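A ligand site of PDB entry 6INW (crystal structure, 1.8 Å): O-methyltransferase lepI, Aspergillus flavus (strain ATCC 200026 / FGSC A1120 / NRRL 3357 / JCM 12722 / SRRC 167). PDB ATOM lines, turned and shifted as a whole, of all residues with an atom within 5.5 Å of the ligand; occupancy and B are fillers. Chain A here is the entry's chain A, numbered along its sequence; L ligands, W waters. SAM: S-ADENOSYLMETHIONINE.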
ATOM      1  N   LEU A 196     -23.746 -27.774 -21.769  1.00  0.00           N
ATOM      2  CA  LEU A 196     -22.655 -27.362 -22.654  1.00  0.00           C
ATOM      3  C   LEU A 196     -22.576 -28.220 -23.907  1.00  0.00           C
ATOM      4  O   LEU A 196     -22.038 -27.766 -24.924  1.00  0.00           O
ATOM      5  CB  LEU A 196     -21.321 -27.417 -21.926  1.00  0.00           C
ATOM      6  CG  LEU A 196     -20.714 -26.114 -21.401  1.00  0.00           C
ATOM      7  CD1 LEU A 196     -19.281 -26.339 -20.976  1.00  0.00           C
ATOM      8  CD2 LEU A 196     -20.798 -25.000 -22.440  1.00  0.00           C
ATOM      9  N   ASP A 228     -10.309 -19.948 -29.472  1.00  0.00           N
ATOM     10  CA  ASP A 228     -11.698 -20.021 -29.022  1.00  0.00           C
ATOM     11  C   ASP A 228     -11.705 -19.785 -27.510  1.00  0.00           C
ATOM     12  O   ASP A 228     -11.499 -20.715 -26.725  1.00  0.00           O
ATOM     13  CB  ASP A 228     -12.284 -21.391 -29.377  1.00  0.00           C
ATOM     14  CG  ASP A 228     -13.799 -21.456 -29.253  1.00  0.00           C
ATOM     15  OD1 ASP A 228     -14.434 -20.447 -28.890  1.00  0.00           O
ATOM     16  OD2 ASP A 228     -14.353 -22.538 -29.531  1.00  0.00           O
ATOM     17  N   ILE A 229     -11.964 -18.547 -27.096  1.00  0.00           N
ATOM     18  CA  ILE A 229     -11.823 -18.146 -25.701  1.00  0.00           C
ATOM     19  C   ILE A 229     -13.119 -18.455 -24.959  1.00  0.00           C
ATOM     20  O   ILE A 229     -14.176 -17.885 -25.272  1.00  0.00           O
ATOM     21  CB  ILE A 229     -11.449 -16.658 -25.589  1.00  0.00           C
ATOM     22  CG1 ILE A 229     -10.171 -16.380 -26.392  1.00  0.00           C
ATOM     23  CG2 ILE A 229     -11.281 -16.261 -24.124  1.00  0.00           C
ATOM     24  CD1 ILE A 229      -9.830 -14.914 -26.519  1.00  0.00           C
ATOM     25  N   GLY A 230     -13.039 -19.321 -23.958  1.00  0.00           N
ATOM     26  CA  GLY A 230     -14.237 -19.845 -23.324  1.00  0.00           C
ATOM     27  C   GLY A 230     -15.041 -20.709 -24.281  1.00  0.00           C
ATOM     28  O   GLY A 230     -16.286 -20.647 -24.272  1.00  0.00           O
ATOM     29  N   GLY A 231     -14.369 -21.528 -25.083  1.00  0.00           N
ATOM     30  CA  GLY A 231     -14.978 -22.299 -26.151  1.00  0.00           C
ATOM     31  C   GLY A 231     -15.768 -23.514 -25.723  1.00  0.00           C
ATOM     32  O   GLY A 231     -16.353 -24.176 -26.589  1.00  0.00           O
ATOM     33  N   GLY A 232     -15.819 -23.828 -24.434  1.00  0.00           N
ATOM     34  CA  GLY A 232     -16.648 -24.914 -23.962  1.00  0.00           C
ATOM     35  C   GLY A 232     -16.203 -26.247 -24.547  1.00  0.00           C
ATOM     36  O   GLY A 232     -15.045 -26.658 -24.393  1.00  0.00           O
ATOM     37  N   MET A 233     -17.118 -26.917 -25.237  1.00  0.00           N
ATOM     38  CA  MET A 233     -16.830 -28.193 -25.897  1.00  0.00           C
ATOM     39  C   MET A 233     -15.984 -28.010 -27.147  1.00  0.00           C
ATOM     40  O   MET A 233     -15.549 -28.983 -27.761  1.00  0.00           O
ATOM     41  CB  MET A 233     -18.138 -28.904 -26.252  1.00  0.00           C
ATOM     42  CG  MET A 233     -18.990 -29.252 -25.042  1.00  0.00           C
ATOM     43  SD  MET A 233     -18.057 -30.449 -23.820  1.00  0.00           S
ATOM     44  CE  MET A 233     -17.479 -29.159 -22.483  1.00  0.00           C
ATOM     45  N   HIS A 235     -17.085 -26.575 -30.004  1.00  0.00           N
ATOM     46  CA  HIS A 235     -17.884 -26.758 -31.206  1.00  0.00           C
ATOM     47  C   HIS A 235     -17.443 -25.805 -32.314  1.00  0.00           C
ATOM     48  O   HIS A 235     -17.415 -26.189 -33.498  1.00  0.00           O
ATOM     49  CB  HIS A 235     -19.369 -26.533 -30.890  1.00  0.00           C
ATOM     50  CG  HIS A 235     -19.944 -27.544 -29.938  1.00  0.00           C
ATOM     51  ND1 HIS A 235     -20.878 -27.221 -28.992  1.00  0.00           N
ATOM     52  CD2 HIS A 235     -19.723 -28.874 -29.817  1.00  0.00           C
ATOM     53  CE1 HIS A 235     -21.204 -28.298 -28.300  1.00  0.00           C
ATOM     54  NE2 HIS A 235     -20.518 -29.319 -28.783  1.00  0.00           N
ATOM     55  N   ALA A 236     -17.112 -24.569 -31.970  1.00  0.00           N
ATOM     56  CA  ALA A 236     -16.667 -23.619 -32.985  1.00  0.00           C
ATOM     57  C   ALA A 236     -15.390 -24.112 -33.670  1.00  0.00           C
ATOM     58  O   ALA A 236     -15.270 -24.037 -34.894  1.00  0.00           O
ATOM     59  CB  ALA A 236     -16.466 -22.235 -32.371  1.00  0.00           C
ATOM     60  N   GLN A 254      -9.688 -22.761 -25.657  1.00  0.00           N
ATOM     61  CA  GLN A 254      -9.313 -22.279 -24.331  1.00  0.00           C
ATOM     62  C   GLN A 254     -10.524 -22.312 -23.410  1.00  0.00           C
ATOM     63  O   GLN A 254     -11.578 -21.756 -23.744  1.00  0.00           O
ATOM     64  CB  GLN A 254      -8.741 -20.859 -24.392  1.00  0.00           C
ATOM     65  CG  GLN A 254      -7.395 -20.761 -25.086  1.00  0.00           C
ATOM     66  CD  GLN A 254      -6.838 -19.340 -25.090  1.00  0.00           C
ATOM     67  OE1 GLN A 254      -7.577 -18.373 -24.920  1.00  0.00           O
ATOM     68  NE2 GLN A 254      -5.535 -19.219 -25.309  1.00  0.00           N
ATOM     69  N   ASP A 255     -10.362 -22.934 -22.250  1.00  0.00           N
ATOM     70  CA  ASP A 255     -11.411 -22.957 -21.226  1.00  0.00           C
ATOM     71  C   ASP A 255     -10.769 -23.405 -19.918  1.00  0.00           C
ATOM     72  O   ASP A 255      -9.547 -23.554 -19.818  1.00  0.00           O
ATOM     73  CB  ASP A 255     -12.564 -23.870 -21.641  1.00  0.00           C
ATOM     74  CG  ASP A 255     -13.904 -23.390 -21.125  1.00  0.00           C
ATOM     75  OD1 ASP A 255     -14.098 -23.367 -19.889  1.00  0.00           O
ATOM     76  OD2 ASP A 255     -14.764 -23.009 -21.948  1.00  0.00           O
ATOM     77  N   LEU A 256     -11.596 -23.597 -18.894  1.00  0.00           N
ATOM     78  CA  LEU A 256     -11.105 -24.060 -17.604  1.00  0.00           C
ATOM     79  C   LEU A 256     -10.889 -25.579 -17.642  1.00  0.00           C
ATOM     80  O   LEU A 256     -11.526 -26.287 -18.432  1.00  0.00           O
ATOM     81  CB  LEU A 256     -12.086 -23.691 -16.506  1.00  0.00           C
ATOM     82  CG  LEU A 256     -12.331 -22.180 -16.346  1.00  0.00           C
ATOM     83  CD1 LEU A 256     -13.250 -21.895 -15.176  1.00  0.00           C
ATOM     84  CD2 LEU A 256     -11.008 -21.410 -16.210  1.00  0.00           C
ATOM     85  N   VAL A 259     -13.799 -28.213 -17.895  1.00  0.00           N
ATOM     86  CA  VAL A 259     -14.498 -28.142 -19.173  1.00  0.00           C
ATOM     87  C   VAL A 259     -13.650 -28.761 -20.287  1.00  0.00           C
ATOM     88  O   VAL A 259     -14.159 -29.497 -21.133  1.00  0.00           O
ATOM     89  CB  VAL A 259     -14.872 -26.679 -19.475  1.00  0.00           C
ATOM     90  CG1 VAL A 259     -15.554 -26.570 -20.842  1.00  0.00           C
ATOM     91  CG2 VAL A 259     -15.764 -26.130 -18.382  1.00  0.00           C
ATOM     92  N   HIS A 277      -6.959 -21.885 -19.886  1.00  0.00           N
ATOM     93  CA  HIS A 277      -6.775 -20.451 -19.794  1.00  0.00           C
ATOM     94  C   HIS A 277      -7.985 -19.816 -19.146  1.00  0.00           C
ATOM     95  O   HIS A 277      -9.120 -20.072 -19.562  1.00  0.00           O
ATOM     96  CB  HIS A 277      -6.534 -19.835 -21.186  1.00  0.00           C
ATOM     97  CG  HIS A 277      -6.498 -18.339 -21.192  1.00  0.00           C
ATOM     98  ND1 HIS A 277      -5.633 -17.616 -20.399  1.00  0.00           N
ATOM     99  CD2 HIS A 277      -7.212 -17.429 -21.891  1.00  0.00           C
ATOM    100  CE1 HIS A 277      -5.812 -16.323 -20.609  1.00  0.00           C
ATOM    101  NE2 HIS A 277      -6.769 -16.181 -21.507  1.00  0.00           N
ATOM    102  N   ASN A 278      -7.740 -18.985 -18.129  1.00  0.00           N
ATOM    103  CA  ASN A 278      -8.778 -18.174 -17.507  1.00  0.00           C
ATOM    104  C   ASN A 278      -8.829 -16.849 -18.255  1.00  0.00           C
ATOM    105  O   ASN A 278      -7.826 -16.128 -18.295  1.00  0.00           O
ATOM    106  CB  ASN A 278      -8.450 -17.983 -16.023  1.00  0.00           C
ATOM    107  CG  ASN A 278      -9.582 -17.335 -15.249  1.00  0.00           C
ATOM    108  OD1 ASN A 278     -10.269 -16.437 -15.741  1.00  0.00           O
ATOM    109  ND2 ASN A 278      -9.781 -17.788 -14.015  1.00  0.00           N
ATOM    110  N   PHE A 279      -9.983 -16.516 -18.835  1.00  0.00           N
ATOM    111  CA  PHE A 279     -10.009 -15.318 -19.670  1.00  0.00           C
ATOM    112  C   PHE A 279     -10.038 -14.035 -18.844  1.00  0.00           C
ATOM    113  O   PHE A 279     -10.131 -12.947 -19.425  1.00  0.00           O
ATOM    114  CB  PHE A 279     -11.169 -15.344 -20.691  1.00  0.00           C
ATOM    115  CG  PHE A 279     -12.550 -15.592 -20.117  1.00  0.00           C
ATOM    116  CD1 PHE A 279     -13.053 -14.829 -19.070  1.00  0.00           C
ATOM    117  CD2 PHE A 279     -13.375 -16.538 -20.703  1.00  0.00           C
ATOM    118  CE1 PHE A 279     -14.337 -15.050 -18.593  1.00  0.00           C
ATOM    119  CE2 PHE A 279     -14.653 -16.764 -20.232  1.00  0.00           C
ATOM    120  CZ  PHE A 279     -15.133 -16.019 -19.170  1.00  0.00           C
ATOM    121  N   HIS A 280      -9.931 -14.129 -17.528  1.00  0.00           N
ATOM    122  CA  HIS A 280      -9.676 -12.972 -16.679  1.00  0.00           C
ATOM    123  C   HIS A 280      -8.191 -12.681 -16.519  1.00  0.00           C
ATOM    124  O   HIS A 280      -7.831 -11.793 -15.744  1.00  0.00           O
ATOM    125  CB  HIS A 280     -10.318 -13.172 -15.301  1.00  0.00           C
ATOM    126  CG  HIS A 280     -11.815 -13.184 -15.332  1.00  0.00           C
ATOM    127  ND1 HIS A 280     -12.558 -12.101 -15.735  1.00  0.00           N
ATOM    128  CD2 HIS A 280     -12.706 -14.153 -15.034  1.00  0.00           C
ATOM    129  CE1 HIS A 280     -13.845 -12.397 -15.676  1.00  0.00           C
ATOM    130  NE2 HIS A 280     -13.965 -13.641 -15.247  1.00  0.00           N
ATOM    131  N   ARG A 294     -17.725 -16.337 -28.153  1.00  0.00           N
ATOM    132  CA  ARG A 294     -19.108 -16.635 -28.491  1.00  0.00           C
ATOM    133  C   ARG A 294     -19.937 -16.812 -27.227  1.00  0.00           C
ATOM    134  O   ARG A 294     -19.659 -17.714 -26.417  1.00  0.00           O
ATOM    135  CB  ARG A 294     -19.231 -17.883 -29.376  1.00  0.00           C
ATOM    136  CG  ARG A 294     -20.674 -18.163 -29.793  1.00  0.00           C
ATOM    137  CD  ARG A 294     -20.753 -19.122 -30.969  1.00  0.00           C
ATOM    138  NE  ARG A 294     -20.372 -20.470 -30.586  1.00  0.00           N
ATOM    139  CZ  ARG A 294     -20.154 -21.465 -31.435  1.00  0.00           C
ATOM    140  NH1 ARG A 294     -20.281 -21.253 -32.741  1.00  0.00           N
ATOM    141  NH2 ARG A 294     -19.804 -22.662 -30.981  1.00  0.00           N
ATOM    142  N   LEU A 295     -20.949 -15.972 -27.063  1.00  0.00           N
ATOM    143  CA  LEU A 295     -21.855 -16.009 -25.911  1.00  0.00           C
ATOM    144  C   LEU A 295     -21.094 -15.929 -24.593  1.00  0.00           C
ATOM    145  O   LEU A 295     -21.443 -16.596 -23.613  1.00  0.00           O
ATOM    146  CB  LEU A 295     -22.747 -17.264 -25.955  1.00  0.00           C
ATOM    147  CG  LEU A 295     -23.720 -17.331 -27.145  1.00  0.00           C
ATOM    148  CD1 LEU A 295     -24.568 -18.603 -27.080  1.00  0.00           C
ATOM    149  CD2 LEU A 295     -24.613 -16.105 -27.190  1.00  0.00           C
ATOM    150  N   ILE A 296     -20.036 -15.127 -24.578  1.00  0.00           N
ATOM    151  CA  ILE A 296     -19.229 -14.925 -23.378  1.00  0.00           C
ATOM    152  C   ILE A 296     -19.581 -13.583 -22.752  1.00  0.00           C
ATOM    153  O   ILE A 296     -20.013 -13.511 -21.589  1.00  0.00           O
ATOM    154  CB  ILE A 296     -17.720 -14.997 -23.687  1.00  0.00           C
ATOM    155  CG1 ILE A 296     -17.339 -16.357 -24.262  1.00  0.00           C
ATOM    156  CG2 ILE A 296     -16.913 -14.680 -22.428  1.00  0.00           C
ATOM    157  CD1 ILE A 296     -17.638 -17.519 -23.341  1.00  0.00           C
ATOM    158  N   ASP A 299     -22.699 -12.368 -20.596  1.00  0.00           N
ATOM    159  CA  ASP A 299     -22.893 -12.798 -19.223  1.00  0.00           C
ATOM    160  C   ASP A 299     -22.210 -11.890 -18.212  1.00  0.00           C
ATOM    161  O   ASP A 299     -22.248 -12.175 -17.011  1.00  0.00           O
ATOM    162  CB  ASP A 299     -22.391 -14.239 -19.044  1.00  0.00           C
ATOM    163  CG  ASP A 299     -23.338 -15.258 -19.650  1.00  0.00           C
ATOM    164  OD1 ASP A 299     -24.449 -14.881 -20.051  1.00  0.00           O
ATOM    165  OD2 ASP A 299     -22.958 -16.456 -19.722  1.00  0.00           O
ATOM    166  N   PHE A 300     -21.621 -10.789 -18.668  1.00  0.00           N
ATOM    167  CA  PHE A 300     -20.877  -9.908 -17.776  1.00  0.00           C
ATOM    168  C   PHE A 300     -21.342  -8.469 -17.933  1.00  0.00           C
ATOM    169  O   PHE A 300     -21.650  -8.032 -19.052  1.00  0.00           O
ATOM    170  CB  PHE A 300     -19.364  -9.990 -18.063  1.00  0.00           C
ATOM    171  CG  PHE A 300     -18.763 -11.333 -17.796  1.00  0.00           C
ATOM    172  CD1 PHE A 300     -18.287 -11.650 -16.534  1.00  0.00           C
ATOM    173  CD2 PHE A 300     -18.667 -12.281 -18.798  1.00  0.00           C
ATOM    174  CE1 PHE A 300     -17.744 -12.893 -16.269  1.00  0.00           C
ATOM    175  CE2 PHE A 300     -18.117 -13.528 -18.540  1.00  0.00           C
ATOM    176  CZ  PHE A 300     -17.651 -13.831 -17.280  1.00  0.00           C
HETATM  177  N   SAM L   1     -18.184 -20.290 -26.352  1.00  0.00           N
HETATM  178  CA  SAM L   1     -19.099 -21.400 -26.140  1.00  0.00           C
HETATM  179  C   SAM L   1     -19.862 -21.758 -27.410  1.00  0.00           C
HETATM  180  O   SAM L   1     -20.568 -20.913 -27.967  1.00  0.00           O
HETATM  181  OXT SAM L   1     -19.798 -22.880 -27.904  1.00  0.00           O
HETATM  182  CB  SAM L   1     -20.089 -21.070 -25.030  1.00  0.00           C
HETATM  183  CG  SAM L   1     -19.709 -21.688 -23.695  1.00  0.00           C
HETATM  184  SD  SAM L   1     -20.724 -21.122 -22.303  1.00  0.00           S
HETATM  185  CE  SAM L   1     -21.766 -19.842 -23.056  1.00  0.00           C
HETATM  186  C5' SAM L   1     -19.498 -20.145 -21.384  1.00  0.00           C
HETATM  187  C4' SAM L   1     -18.131 -20.819 -21.355  1.00  0.00           C
HETATM  188  O4' SAM L   1     -17.171 -19.989 -20.731  1.00  0.00           O
HETATM  189  C3' SAM L   1     -18.155 -22.120 -20.573  1.00  0.00           C
HETATM  190  O3' SAM L   1     -17.583 -23.126 -21.377  1.00  0.00           O
HETATM  191  C2' SAM L   1     -17.286 -21.878 -19.364  1.00  0.00           C
HETATM  192  O2' SAM L   1     -16.554 -23.026 -18.997  1.00  0.00           O
HETATM  193  C1' SAM L   1     -16.373 -20.774 -19.853  1.00  0.00           C
HETATM  194  N9  SAM L   1     -15.802 -19.966 -18.781  1.00  0.00           N
HETATM  195  C8  SAM L   1     -16.437 -19.446 -17.681  1.00  0.00           C
HETATM  196  N7  SAM L   1     -15.527 -18.748 -16.950  1.00  0.00           N
HETATM  197  C5  SAM L   1     -14.331 -18.822 -17.583  1.00  0.00           C
HETATM  198  C6  SAM L   1     -13.076 -18.301 -17.286  1.00  0.00           C
HETATM  199  N6  SAM L   1     -12.902 -17.564 -16.189  1.00  0.00           N
HETATM  200  N1  SAM L   1     -12.026 -18.542 -18.135  1.00  0.00           N
HETATM  201  C2  SAM L   1     -12.201 -19.304 -19.266  1.00  0.00           C
HETATM  202  N3  SAM L   1     -13.446 -19.818 -19.556  1.00  0.00           N
HETATM  203  C4  SAM L   1     -14.489 -19.581 -18.728  1.00  0.00           C
HETATM  204  O   HOH W   1     -16.833 -23.503 -16.105  1.00  0.00           O
HETATM  205  O   HOH W   2     -23.164 -21.113 -28.663  1.00  0.00           O
HETATM  206  O   HOH W   3     -19.700 -20.133 -17.346  1.00  0.00           O
HETATM  207  O   HOH W   4     -18.763 -24.441 -17.574  1.00  0.00           O
HETATM  208  O   HOH W   5     -18.534 -25.528 -27.915  1.00  0.00           O
HETATM  209  O   HOH W   6     -20.653 -17.088 -20.874  1.00  0.00           O
HETATM  210  O   HOH W   7     -17.225 -17.045 -15.406  1.00  0.00           O
HETATM  211  O   HOH W   8     -18.481 -17.325 -19.691  1.00  0.00           O
HETATM  212  O   HOH W   9     -21.566 -24.766 -28.636  1.00  0.00           O
HETATM  213  O   HOH W  10     -23.935 -17.222 -22.321  1.00  0.00           O
HETATM  214  O   HOH W  11     -15.907 -18.600 -27.263  1.00  0.00           O
HETATM  215  O   HOH W  12     -17.140 -20.910 -28.990  1.00  0.00           O
HETATM  216  O   HOH W  13     -14.379 -17.354 -13.683  1.00  0.00           O
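The side-chain carboxylate of Asp 255 is in hydrogen-bond range of an oxygen (O2') of the ligand.
A nitrogen (N) of the ligand sits at hydrogen-bond distance from the backbone carbonyl oxygen of Gly 230, at 2.8 Å.
The guanidinium group of Arg 294 is in salt-bridge range of an oxygen (O) of the ligand.
The backbone carbonyl oxygen (O) of Arg 294 sits at hydrogen-bond distance from a nitrogen (N) of the ligand, at 3.0 Å.
A nitrogen (N1) of the ligand lies within hydrogen-bond range of the backbone NH of Phe 279.
The side-chain amide oxygen (OD1) of Asn 278 sits at hydrogen-bond distance from a nitrogen (N6) of the ligand, at 2.9 Å.
N of Gly 231 is in hydrogen-bond range of O of Gln 254 (3.1 Å).
The side-chain carboxylate of Asp 255 lies within hydrogen-bond range of the backbone NH of Gly 231.
O of Gln 254 lies within hydrogen-bond range of N of Gly 230.
The side-chain amide oxygen (OD1) of Asn 278 sits at hydrogen-bond distance from the backbone NH (N) of His 280 (2.9 Å).
The side-chain carboxylate of Asp 255 is in hydrogen-bond range of the backbone NH of Gly 232 (2.8 Å).
The backbone carbonyl oxygen (O) of Asp 255 lies within hydrogen-bond range of the backbone NH (N) of His 277, at 3.1 Å.
Leu 196 touches the ligand.
Gly 231 touches the ligand (CA to N, 3.8 Å).
CA of Gly 232 touches O3' of the ligand, 3.3 Å away.
Leu 256 touches the ligand.
Val 259 touches the ligand (CG2 to O2', 3.3 Å).
O of His 277 touches C2 of the ligand, at 3.2 Å.
His 280 touches the ligand (CD2 to N6, 3.6 Å).
Leu 295 touches the ligand (O to CE, 3.3 Å).
CD1 of Ile 296 touches O4' of the ligand, at 3.6 Å.
Hydrophobic or aromatic side chains that line the ligand: Leu 196, Leu 256, Val 259, Phe 279, His 280 and Ile 296.
14 residues have an atom within 4 Å of the ligand: Leu 196, Gly 230, Gly 231, Gly 232, Asp 255, Leu 256, Val 259, His 277, Asn 278, Phe 279, His 280, Arg 294, Leu 295 and Ile 296.
The nearest printed residue that does not touch the ligand is Asp 228 (4.5 Å).
Water W2 lies within hydrogen-bond range of O of the ligand (2.7 Å) and NE of Arg 294 (3.5 Å).
Water W12 lies within hydrogen-bond range of the side-chain carboxylate of Asp 228 and a nitrogen (N) of the ligand.
Water W5 lies within hydrogen-bond range of the backbone NH of His 235 (2.7 Å), the backbone carbonyl oxygen of Gly 231 (2.9 Å), an oxygen (OXT) of the ligand (2.9 Å) and the backbone NH of Met 233 (3.3 Å).
Water W11 lies within hydrogen-bond range of O of Ile 229, OD1 of Asp 228, N of the ligand and N of Arg 294.
Water W6 lies within hydrogen-bond range of OD2 of Asp 299 (2.7 Å) and O of Leu 295 (2.9 Å).
Water W10 lies within hydrogen-bond range of the backbone carbonyl oxygen (O) of Leu 295 (2.9 Å) and the side-chain carboxylate (OD2) of Asp 299 (2.9 Å).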
